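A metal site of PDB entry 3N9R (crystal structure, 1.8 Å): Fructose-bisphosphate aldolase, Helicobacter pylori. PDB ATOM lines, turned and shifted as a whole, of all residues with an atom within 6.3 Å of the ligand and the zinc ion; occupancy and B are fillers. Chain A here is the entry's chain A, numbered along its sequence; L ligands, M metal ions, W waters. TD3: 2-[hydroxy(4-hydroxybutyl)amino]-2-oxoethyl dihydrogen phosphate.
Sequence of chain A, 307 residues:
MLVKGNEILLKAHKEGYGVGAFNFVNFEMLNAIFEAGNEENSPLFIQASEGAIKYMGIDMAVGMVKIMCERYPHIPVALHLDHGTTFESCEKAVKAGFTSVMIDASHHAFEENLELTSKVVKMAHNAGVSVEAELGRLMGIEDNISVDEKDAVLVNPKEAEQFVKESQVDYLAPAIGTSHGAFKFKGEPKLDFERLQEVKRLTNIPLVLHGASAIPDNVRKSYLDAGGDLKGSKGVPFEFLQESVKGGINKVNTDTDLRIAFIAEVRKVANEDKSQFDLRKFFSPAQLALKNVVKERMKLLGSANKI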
ATOM      1  N   ASN A  23     -28.731 -15.946 -25.506  1.00  0.00           N
ATOM      2  CA  ASN A  23     -27.512 -15.287 -25.933  1.00  0.00           C
ATOM      3  C   ASN A  23     -27.800 -14.035 -26.778  1.00  0.00           C
ATOM      4  O   ASN A  23     -28.764 -13.988 -27.533  1.00  0.00           O
ATOM      5  CB  ASN A  23     -26.653 -16.260 -26.752  1.00  0.00           C
ATOM      6  CG  ASN A  23     -25.948 -17.269 -25.870  1.00  0.00           C
ATOM      7  OD1 ASN A  23     -26.556 -18.234 -25.423  1.00  0.00           O
ATOM      8  ND2 ASN A  23     -24.670 -17.041 -25.612  1.00  0.00           N
ATOM      9  N   GLN A  47     -27.170 -13.842 -21.792  1.00  0.00           N
ATOM     10  CA  GLN A  47     -25.864 -14.503 -21.806  1.00  0.00           C
ATOM     11  C   GLN A  47     -24.998 -13.943 -22.886  1.00  0.00           C
ATOM     12  O   GLN A  47     -25.490 -13.635 -23.977  1.00  0.00           O
ATOM     13  CB  GLN A  47     -25.982 -15.996 -22.110  1.00  0.00           C
ATOM     14  CG  GLN A  47     -26.942 -16.740 -21.248  1.00  0.00           C
ATOM     15  CD  GLN A  47     -26.690 -18.225 -21.307  1.00  0.00           C
ATOM     16  OE1 GLN A  47     -26.481 -18.851 -20.279  1.00  0.00           O
ATOM     17  NE2 GLN A  47     -26.706 -18.797 -22.499  1.00  0.00           N
ATOM     18  N   ASP A  82     -21.296 -17.010 -20.646  1.00  0.00           N
ATOM     19  CA  ASP A  82     -21.560 -18.341 -21.161  1.00  0.00           C
ATOM     20  C   ASP A  82     -20.212 -18.997 -21.602  1.00  0.00           C
ATOM     21  O   ASP A  82     -19.429 -18.376 -22.325  1.00  0.00           O
ATOM     22  CB  ASP A  82     -22.515 -18.181 -22.350  1.00  0.00           C
ATOM     23  CG  ASP A  82     -23.032 -19.490 -22.889  1.00  0.00           C
ATOM     24  OD1 ASP A  82     -23.066 -20.479 -22.138  1.00  0.00           O
ATOM     25  OD2 ASP A  82     -23.433 -19.516 -24.083  1.00  0.00           O
ATOM     26  N   HIS A  83     -19.946 -20.202 -21.121  1.00  0.00           N
ATOM     27  CA  HIS A  83     -18.764 -20.986 -21.492  1.00  0.00           C
ATOM     28  C   HIS A  83     -17.452 -20.227 -21.297  1.00  0.00           C
ATOM     29  O   HIS A  83     -16.632 -20.125 -22.205  1.00  0.00           O
ATOM     30  CB  HIS A  83     -18.874 -21.482 -22.945  1.00  0.00           C
ATOM     31  CG  HIS A  83     -19.919 -22.540 -23.123  1.00  0.00           C
ATOM     32  ND1 HIS A  83     -19.749 -23.833 -22.675  1.00  0.00           N
ATOM     33  CD2 HIS A  83     -21.162 -22.488 -23.665  1.00  0.00           C
ATOM     34  CE1 HIS A  83     -20.834 -24.540 -22.950  1.00  0.00           C
ATOM     35  NE2 HIS A  83     -21.696 -23.742 -23.549  1.00  0.00           N
ATOM     36  N   MET A 102     -20.057 -18.798 -16.047  1.00  0.00           N
ATOM     37  CA  MET A 102     -19.859 -20.224 -16.183  1.00  0.00           C
ATOM     38  C   MET A 102     -18.384 -20.511 -16.419  1.00  0.00           C
ATOM     39  O   MET A 102     -17.784 -19.919 -17.310  1.00  0.00           O
ATOM     40  CB  MET A 102     -20.635 -20.791 -17.385  1.00  0.00           C
ATOM     41  CG  MET A 102     -20.436 -22.296 -17.526  1.00  0.00           C
ATOM     42  SD  MET A 102     -20.845 -22.878 -19.173  1.00  0.00           S
ATOM     43  CE  MET A 102     -20.904 -24.634 -18.875  1.00  0.00           C
ATOM     44  N   GLU A 134     -19.818 -27.396 -15.274  1.00  0.00           N
ATOM     45  CA  GLU A 134     -20.373 -28.441 -16.149  1.00  0.00           C
ATOM     46  C   GLU A 134     -19.733 -29.804 -15.879  1.00  0.00           C
ATOM     47  O   GLU A 134     -18.523 -29.897 -15.673  1.00  0.00           O
ATOM     48  CB  GLU A 134     -20.176 -28.080 -17.632  1.00  0.00           C
ATOM     49  CG  GLU A 134     -20.804 -29.079 -18.604  1.00  0.00           C
ATOM     50  CD  GLU A 134     -20.720 -28.640 -20.064  1.00  0.00           C
ATOM     51  OE1 GLU A 134     -19.776 -27.921 -20.446  1.00  0.00           O
ATOM     52  OE2 GLU A 134     -21.618 -28.992 -20.856  1.00  0.00           O
ATOM     53  N   LEU A 138     -21.377 -33.082 -23.554  1.00  0.00           N
ATOM     54  CA  LEU A 138     -22.556 -32.712 -24.325  1.00  0.00           C
ATOM     55  C   LEU A 138     -22.544 -33.375 -25.694  1.00  0.00           C
ATOM     56  O   LEU A 138     -21.892 -32.905 -26.614  1.00  0.00           O
ATOM     57  CB  LEU A 138     -22.596 -31.203 -24.493  1.00  0.00           C
ATOM     58  CG  LEU A 138     -23.939 -30.499 -24.283  1.00  0.00           C
ATOM     59  CD1 LEU A 138     -24.571 -30.861 -22.945  1.00  0.00           C
ATOM     60  CD2 LEU A 138     -23.717 -29.002 -24.384  1.00  0.00           C
ATOM     61  N   SER A 179     -26.926 -31.456 -27.228  1.00  0.00           N
ATOM     62  CA  SER A 179     -25.665 -30.968 -27.777  1.00  0.00           C
ATOM     63  C   SER A 179     -25.927 -29.598 -28.374  1.00  0.00           C
ATOM     64  O   SER A 179     -27.075 -29.244 -28.641  1.00  0.00           O
ATOM     65  CB  SER A 179     -25.129 -31.921 -28.848  1.00  0.00           C
ATOM     66  OG  SER A 179     -26.154 -32.328 -29.726  1.00  0.00           O
ATOM     67  N   HIS A 180     -24.870 -28.818 -28.584  1.00  0.00           N
ATOM     68  CA  HIS A 180     -25.019 -27.493 -29.143  1.00  0.00           C
ATOM     69  C   HIS A 180     -25.411 -27.524 -30.615  1.00  0.00           C
ATOM     70  O   HIS A 180     -25.029 -28.434 -31.339  1.00  0.00           O
ATOM     71  CB  HIS A 180     -23.697 -26.738 -29.015  1.00  0.00           C
ATOM     72  CG  HIS A 180     -23.356 -26.385 -27.592  1.00  0.00           C
ATOM     73  ND1 HIS A 180     -22.088 -26.539 -27.074  1.00  0.00           N
ATOM     74  CD2 HIS A 180     -24.119 -25.883 -26.595  1.00  0.00           C
ATOM     75  CE1 HIS A 180     -22.085 -26.151 -25.812  1.00  0.00           C
ATOM     76  NE2 HIS A 180     -23.304 -25.744 -25.496  1.00  0.00           N
ATOM     77  N   GLY A 181     -26.144 -26.503 -31.058  1.00  0.00           N
ATOM     78  CA  GLY A 181     -26.380 -26.283 -32.477  1.00  0.00           C
ATOM     79  C   GLY A 181     -27.652 -26.874 -33.041  1.00  0.00           C
ATOM     80  O   GLY A 181     -28.472 -27.426 -32.318  1.00  0.00           O
ATOM     81  N   ALA A 182     -27.821 -26.782 -34.364  1.00  0.00           N
ATOM     82  CA  ALA A 182     -29.101 -27.133 -34.977  1.00  0.00           C
ATOM     83  C   ALA A 182     -29.249 -28.639 -35.279  1.00  0.00           C
ATOM     84  O   ALA A 182     -30.319 -29.058 -35.718  1.00  0.00           O
ATOM     85  CB  ALA A 182     -29.324 -26.298 -36.251  1.00  0.00           C
ATOM     86  N   LYS A 184     -29.045 -31.805 -33.419  1.00  0.00           N
ATOM     87  CA  LYS A 184     -28.868 -32.454 -32.125  1.00  0.00           C
ATOM     88  C   LYS A 184     -29.106 -33.950 -32.179  1.00  0.00           C
ATOM     89  O   LYS A 184     -28.588 -34.690 -31.340  1.00  0.00           O
ATOM     90  CB  LYS A 184     -29.777 -31.844 -31.059  1.00  0.00           C
ATOM     91  CG  LYS A 184     -29.686 -30.324 -30.972  1.00  0.00           C
ATOM     92  CD  LYS A 184     -30.446 -29.773 -29.750  1.00  0.00           C
ATOM     93  CE  LYS A 184     -30.455 -28.238 -29.786  1.00  0.00           C
ATOM     94  NZ  LYS A 184     -29.068 -27.673 -29.711  1.00  0.00           N
ATOM     95  N   LEU A 209     -29.549 -26.674 -18.512  1.00  0.00           N
ATOM     96  CA  LEU A 209     -29.578 -27.468 -19.743  1.00  0.00           C
ATOM     97  C   LEU A 209     -28.944 -26.693 -20.876  1.00  0.00           C
ATOM     98  O   LEU A 209     -29.483 -25.678 -21.322  1.00  0.00           O
ATOM     99  CB  LEU A 209     -31.023 -27.826 -20.100  1.00  0.00           C
ATOM    100  CG  LEU A 209     -31.171 -28.843 -21.240  1.00  0.00           C
ATOM    101  CD1 LEU A 209     -30.590 -30.179 -20.823  1.00  0.00           C
ATOM    102  CD2 LEU A 209     -32.646 -28.981 -21.612  1.00  0.00           C
ATOM    103  N   HIS A 210     -27.802 -27.168 -21.369  1.00  0.00           N
ATOM    104  CA  HIS A 210     -27.163 -26.559 -22.536  1.00  0.00           C
ATOM    105  C   HIS A 210     -27.746 -27.208 -23.772  1.00  0.00           C
ATOM    106  O   HIS A 210     -28.312 -28.292 -23.685  1.00  0.00           O
ATOM    107  CB  HIS A 210     -25.663 -26.770 -22.493  1.00  0.00           C
ATOM    108  CG  HIS A 210     -24.960 -25.803 -21.600  1.00  0.00           C
ATOM    109  ND1 HIS A 210     -24.097 -24.851 -22.076  1.00  0.00           N
ATOM    110  CD2 HIS A 210     -25.058 -25.607 -20.258  1.00  0.00           C
ATOM    111  CE1 HIS A 210     -23.649 -24.125 -21.066  1.00  0.00           C
ATOM    112  NE2 HIS A 210     -24.223 -24.571 -19.954  1.00  0.00           N
ATOM    113  N   GLY A 211     -27.610 -26.542 -24.912  1.00  0.00           N
ATOM    114  CA  GLY A 211     -28.039 -27.133 -26.180  1.00  0.00           C
ATOM    115  C   GLY A 211     -29.527 -27.362 -26.213  1.00  0.00           C
ATOM    116  O   GLY A 211     -29.983 -28.395 -26.722  1.00  0.00           O
ATOM    117  N   ALA A 212     -30.291 -26.393 -25.672  1.00  0.00           N
ATOM    118  CA  ALA A 212     -31.726 -26.564 -25.472  1.00  0.00           C
ATOM    119  C   ALA A 212     -32.625 -25.963 -26.556  1.00  0.00           C
ATOM    120  O   ALA A 212     -33.849 -25.909 -26.391  1.00  0.00           O
ATOM    121  CB  ALA A 212     -32.136 -25.996 -24.096  1.00  0.00           C
ATOM    122  N   SER A 213     -32.052 -25.526 -27.674  1.00  0.00           N
ATOM    123  CA  SER A 213     -32.908 -24.990 -28.745  1.00  0.00           C
ATOM    124  C   SER A 213     -33.862 -26.064 -29.260  1.00  0.00           C
ATOM    125  O   SER A 213     -33.522 -27.241 -29.262  1.00  0.00           O
ATOM    126  CB  SER A 213     -32.059 -24.432 -29.899  1.00  0.00           C
ATOM    127  OG  SER A 213     -31.551 -23.162 -29.546  1.00  0.00           O
ATOM    128  N   ALA A 214     -35.052 -25.648 -29.684  1.00  0.00           N
ATOM    129  CA  ALA A 214     -36.078 -26.578 -30.168  1.00  0.00           C
ATOM    130  C   ALA A 214     -36.166 -26.698 -31.697  1.00  0.00           C
ATOM    131  O   ALA A 214     -36.689 -27.685 -32.208  1.00  0.00           O
ATOM    132  CB  ALA A 214     -37.438 -26.134 -29.631  1.00  0.00           C
ATOM    133  N   VAL A 236     -34.472 -29.945 -29.623  1.00  0.00           N
ATOM    134  CA  VAL A 236     -35.110 -30.640 -28.509  1.00  0.00           C
ATOM    135  C   VAL A 236     -36.616 -30.422 -28.600  1.00  0.00           C
ATOM    136  O   VAL A 236     -37.061 -29.298 -28.688  1.00  0.00           O
ATOM    137  CB  VAL A 236     -34.626 -30.117 -27.127  1.00  0.00           C
ATOM    138  CG1 VAL A 236     -35.248 -30.936 -26.001  1.00  0.00           C
ATOM    139  CG2 VAL A 236     -33.088 -30.160 -27.014  1.00  0.00           C
ATOM    140  N   ASN A 253     -30.487 -22.952 -21.742  1.00  0.00           N
ATOM    141  CA  ASN A 253     -29.678 -22.143 -22.656  1.00  0.00           C
ATOM    142  C   ASN A 253     -30.208 -22.227 -24.065  1.00  0.00           C
ATOM    143  O   ASN A 253     -30.313 -23.296 -24.620  1.00  0.00           O
ATOM    144  CB  ASN A 253     -28.232 -22.616 -22.685  1.00  0.00           C
ATOM    145  CG  ASN A 253     -27.492 -22.284 -21.424  1.00  0.00           C
ATOM    146  OD1 ASN A 253     -28.088 -22.074 -20.368  1.00  0.00           O
ATOM    147  ND2 ASN A 253     -26.156 -22.238 -21.520  1.00  0.00           N
ATOM    148  N   THR A 254     -30.473 -21.061 -24.654  1.00  0.00           N
ATOM    149  CA  THR A 254     -31.140 -21.011 -25.942  1.00  0.00           C
ATOM    150  C   THR A 254     -30.484 -19.943 -26.805  1.00  0.00           C
ATOM    151  O   THR A 254     -30.467 -18.778 -26.447  1.00  0.00           O
ATOM    152  CB  THR A 254     -32.616 -20.670 -25.756  1.00  0.00           C
ATOM    153  OG1 THR A 254     -33.172 -21.505 -24.736  1.00  0.00           O
ATOM    154  CG2 THR A 254     -33.381 -20.879 -27.065  1.00  0.00           C
ATOM    155  N   ASP A 255     -29.973 -20.348 -27.966  1.00  0.00           N
ATOM    156  CA  ASP A 255     -29.224 -19.457 -28.825  1.00  0.00           C
ATOM    157  C   ASP A 255     -29.572 -19.725 -30.292  1.00  0.00           C
ATOM    158  O   ASP A 255     -30.046 -18.842 -30.982  1.00  0.00           O
ATOM    159  CB  ASP A 255     -27.721 -19.644 -28.572  1.00  0.00           C
ATOM    160  CG  ASP A 255     -26.843 -18.665 -29.341  1.00  0.00           C
ATOM    161  OD1 ASP A 255     -27.355 -17.845 -30.138  1.00  0.00           O
ATOM    162  OD2 ASP A 255     -25.609 -18.723 -29.134  1.00  0.00           O
ATOM    163  N   THR A 256     -29.383 -20.952 -30.754  1.00  0.00           N
ATOM    164  CA  THR A 256     -29.657 -21.319 -32.154  1.00  0.00           C
ATOM    165  C   THR A 256     -31.062 -20.915 -32.624  1.00  0.00           C
ATOM    166  O   THR A 256     -31.223 -20.345 -33.710  1.00  0.00           O
ATOM    167  CB  THR A 256     -29.402 -22.816 -32.364  1.00  0.00           C
ATOM    168  OG1 THR A 256     -28.003 -23.075 -32.169  1.00  0.00           O
ATOM    169  CG2 THR A 256     -29.824 -23.268 -33.781  1.00  0.00           C
ATOM    170  N   ASP A 257     -32.080 -21.177 -31.824  1.00  0.00           N
ATOM    171  CA  ASP A 257     -33.443 -20.780 -32.204  1.00  0.00           C
ATOM    172  C   ASP A 257     -33.536 -19.306 -32.507  1.00  0.00           C
ATOM    173  O   ASP A 257     -34.190 -18.898 -33.478  1.00  0.00           O
ATOM    174  CB  ASP A 257     -34.439 -21.078 -31.076  1.00  0.00           C
ATOM    175  CG  ASP A 257     -34.825 -22.519 -31.034  1.00  0.00           C
ATOM    176  OD1 ASP A 257     -34.440 -23.269 -31.962  1.00  0.00           O
ATOM    177  OD2 ASP A 257     -35.507 -22.901 -30.066  1.00  0.00           O
ATOM    178  N   ARG A 259     -31.100 -17.243 -33.410  1.00  0.00           N
ATOM    179  CA  ARG A 259     -30.360 -16.918 -34.628  1.00  0.00           C
ATOM    180  C   ARG A 259     -31.174 -17.275 -35.887  1.00  0.00           C
ATOM    181  O   ARG A 259     -31.256 -16.483 -36.818  1.00  0.00           O
ATOM    182  CB  ARG A 259     -29.041 -17.689 -34.691  1.00  0.00           C
ATOM    183  CG  ARG A 259     -28.043 -17.385 -33.569  1.00  0.00           C
ATOM    184  CD  ARG A 259     -26.819 -18.293 -33.736  1.00  0.00           C
ATOM    185  NE  ARG A 259     -25.938 -18.219 -32.587  1.00  0.00           N
ATOM    186  CZ  ARG A 259     -24.645 -18.543 -32.616  1.00  0.00           C
ATOM    187  NH1 ARG A 259     -24.081 -18.952 -33.751  1.00  0.00           N
ATOM    188  NH2 ARG A 259     -23.920 -18.445 -31.511  1.00  0.00           N
HETATM  189  O01 TD3 L   1     -23.610 -22.984 -25.550  1.00  0.00           O
HETATM  190  N02 TD3 L   1     -24.878 -22.725 -26.104  1.00  0.00           N
HETATM  191  C03 TD3 L   1     -24.933 -21.956 -27.341  1.00  0.00           C
HETATM  192  C04 TD3 L   1     -24.221 -22.560 -28.555  1.00  0.00           C
HETATM  193  C05 TD3 L   1     -24.792 -22.357 -29.956  1.00  0.00           C
HETATM  194  C06 TD3 L   1     -24.317 -23.345 -31.028  1.00  0.00           C
HETATM  195  O07 TD3 L   1     -23.619 -22.857 -32.130  1.00  0.00           O
HETATM  196  C12 TD3 L   1     -26.078 -23.350 -25.559  1.00  0.00           C
HETATM  197  O13 TD3 L   1     -25.956 -24.192 -24.717  1.00  0.00           O
HETATM  198  C14 TD3 L   1     -27.325 -23.333 -26.445  1.00  0.00           C
HETATM  199  O15 TD3 L   1     -27.265 -24.213 -27.515  1.00  0.00           O
HETATM  200  P16 TD3 L   1     -28.353 -24.199 -28.756  1.00  0.00           P
HETATM  201  O17 TD3 L   1     -29.420 -25.398 -28.477  1.00  0.00           O
HETATM  202  O18 TD3 L   1     -27.531 -24.425 -30.144  1.00  0.00           O
HETATM  203  O19 TD3 L   1     -29.029 -22.905 -28.840  1.00  0.00           O
HETATM  204 ZN    ZN M   1     -23.684 -24.311 -24.036  1.00  0.00          ZN
HETATM  205  O   HOH W   1     -23.096 -25.593 -32.589  1.00  0.00           O
HETATM  206  O   HOH W   2     -25.991 -22.609 -34.097  1.00  0.00           O
HETATM  207  O   HOH W   3     -25.999 -20.758 -24.637  1.00  0.00           O
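The backbone NH (N) of Thr 256 sits at hydrogen-bond distance from an oxygen (O19) of the ligand (2.8 Å).
The side-chain hydroxyl (OG1) of Thr 256 is in hydrogen-bond range of an oxygen (O18) of the ligand (2.5 Å).
An oxygen (O17) of the ligand lies within salt-bridge range of the side-chain amino group of Lys 184 (2.6 Å).
N of Ser 213 lies within hydrogen-bond range of O17 of the ligand, 2.8 Å away.
O19 of the ligand lies within hydrogen-bond range of OG of Ser 213 (2.6 Å).
The backbone NH of Gly 181 is in hydrogen-bond range of an oxygen (O18) of the ligand, 2.7 Å away.
N of Asp 255 sits at hydrogen-bond distance from O19 of the ligand (2.9 Å).
An oxygen (O13) of the ligand lies close to the backbone NH of Gly 211.
The backbone NH (N) of Ala 212 lies within hydrogen-bond range of an oxygen (O17) of the ligand, at 3.1 Å.
The side-chain sulfur of Met 102 is in hydrogen-bond range of the backbone NH of His 83, at 3.4 Å.
N of Thr 256 sits at hydrogen-bond distance from OG of Ser 213 (3.3 Å).
The backbone carbonyl oxygen of Gly 181 lies within hydrogen-bond range of the side-chain amino group of Lys 184, 2.7 Å away.
NZ of Lys 184 lies close to O of Gly 211 (3.2 Å).
The side-chain amino group (NZ) of Lys 184 is in hydrogen-bond range of the backbone carbonyl oxygen (O) of Ser 179, 2.8 Å away.
The side-chain hydroxyl (OG) of Ser 213 sits at hydrogen-bond distance from the backbone NH (N) of Asp 257.
The guanidinium group (NE) of Arg 259 lies within salt-bridge range of the side-chain carboxylate (OD1) of Asp 255, 2.9 Å away.
The backbone carbonyl oxygen (O) of Asn 253 sits at hydrogen-bond distance from the backbone NH (N) of Ala 212 (3.3 Å).
Residues that only touch the ligand: Asp 82 (3.8 Å), Asn 253 (3.4 Å) and Thr 254 (3.9 Å).
Of the 25 residues printed, 13 come within 4 Å of the ligand.
The nearest printed residue that does not touch the ligand is Arg 259 (4.3 Å).
Of the 25 residues printed, 3 come within 4 Å of the zinc ion.
The nearest printed residue that does not touch the zinc ion is Asn 253 (4.1 Å).
The zinc ion is bound by an oxygen (O01) of the ligand (2.0 Å), a ring nitrogen (ND1) of His 210 (2.1 Å), a ring nitrogen (NE2) of His 180 (2.1 Å), a ring nitrogen (NE2) of His 83 (2.1 Å) and an oxygen (O13) of the ligand (2.4 Å).
The zinc ion has five donor atoms within binding distance.
Water W3 lies within hydrogen-bond range of OD1 of Asn 23 (2.7 Å), OD2 of Asp 82 (2.9 Å), NE2 of Gln 47 (3.0 Å) and ND2 of Asn 253 (3.5 Å).
Water W2 lies within hydrogen-bond range of OG1 of Thr 256 (2.8 Å) and O07 of the ligand (3.1 Å).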
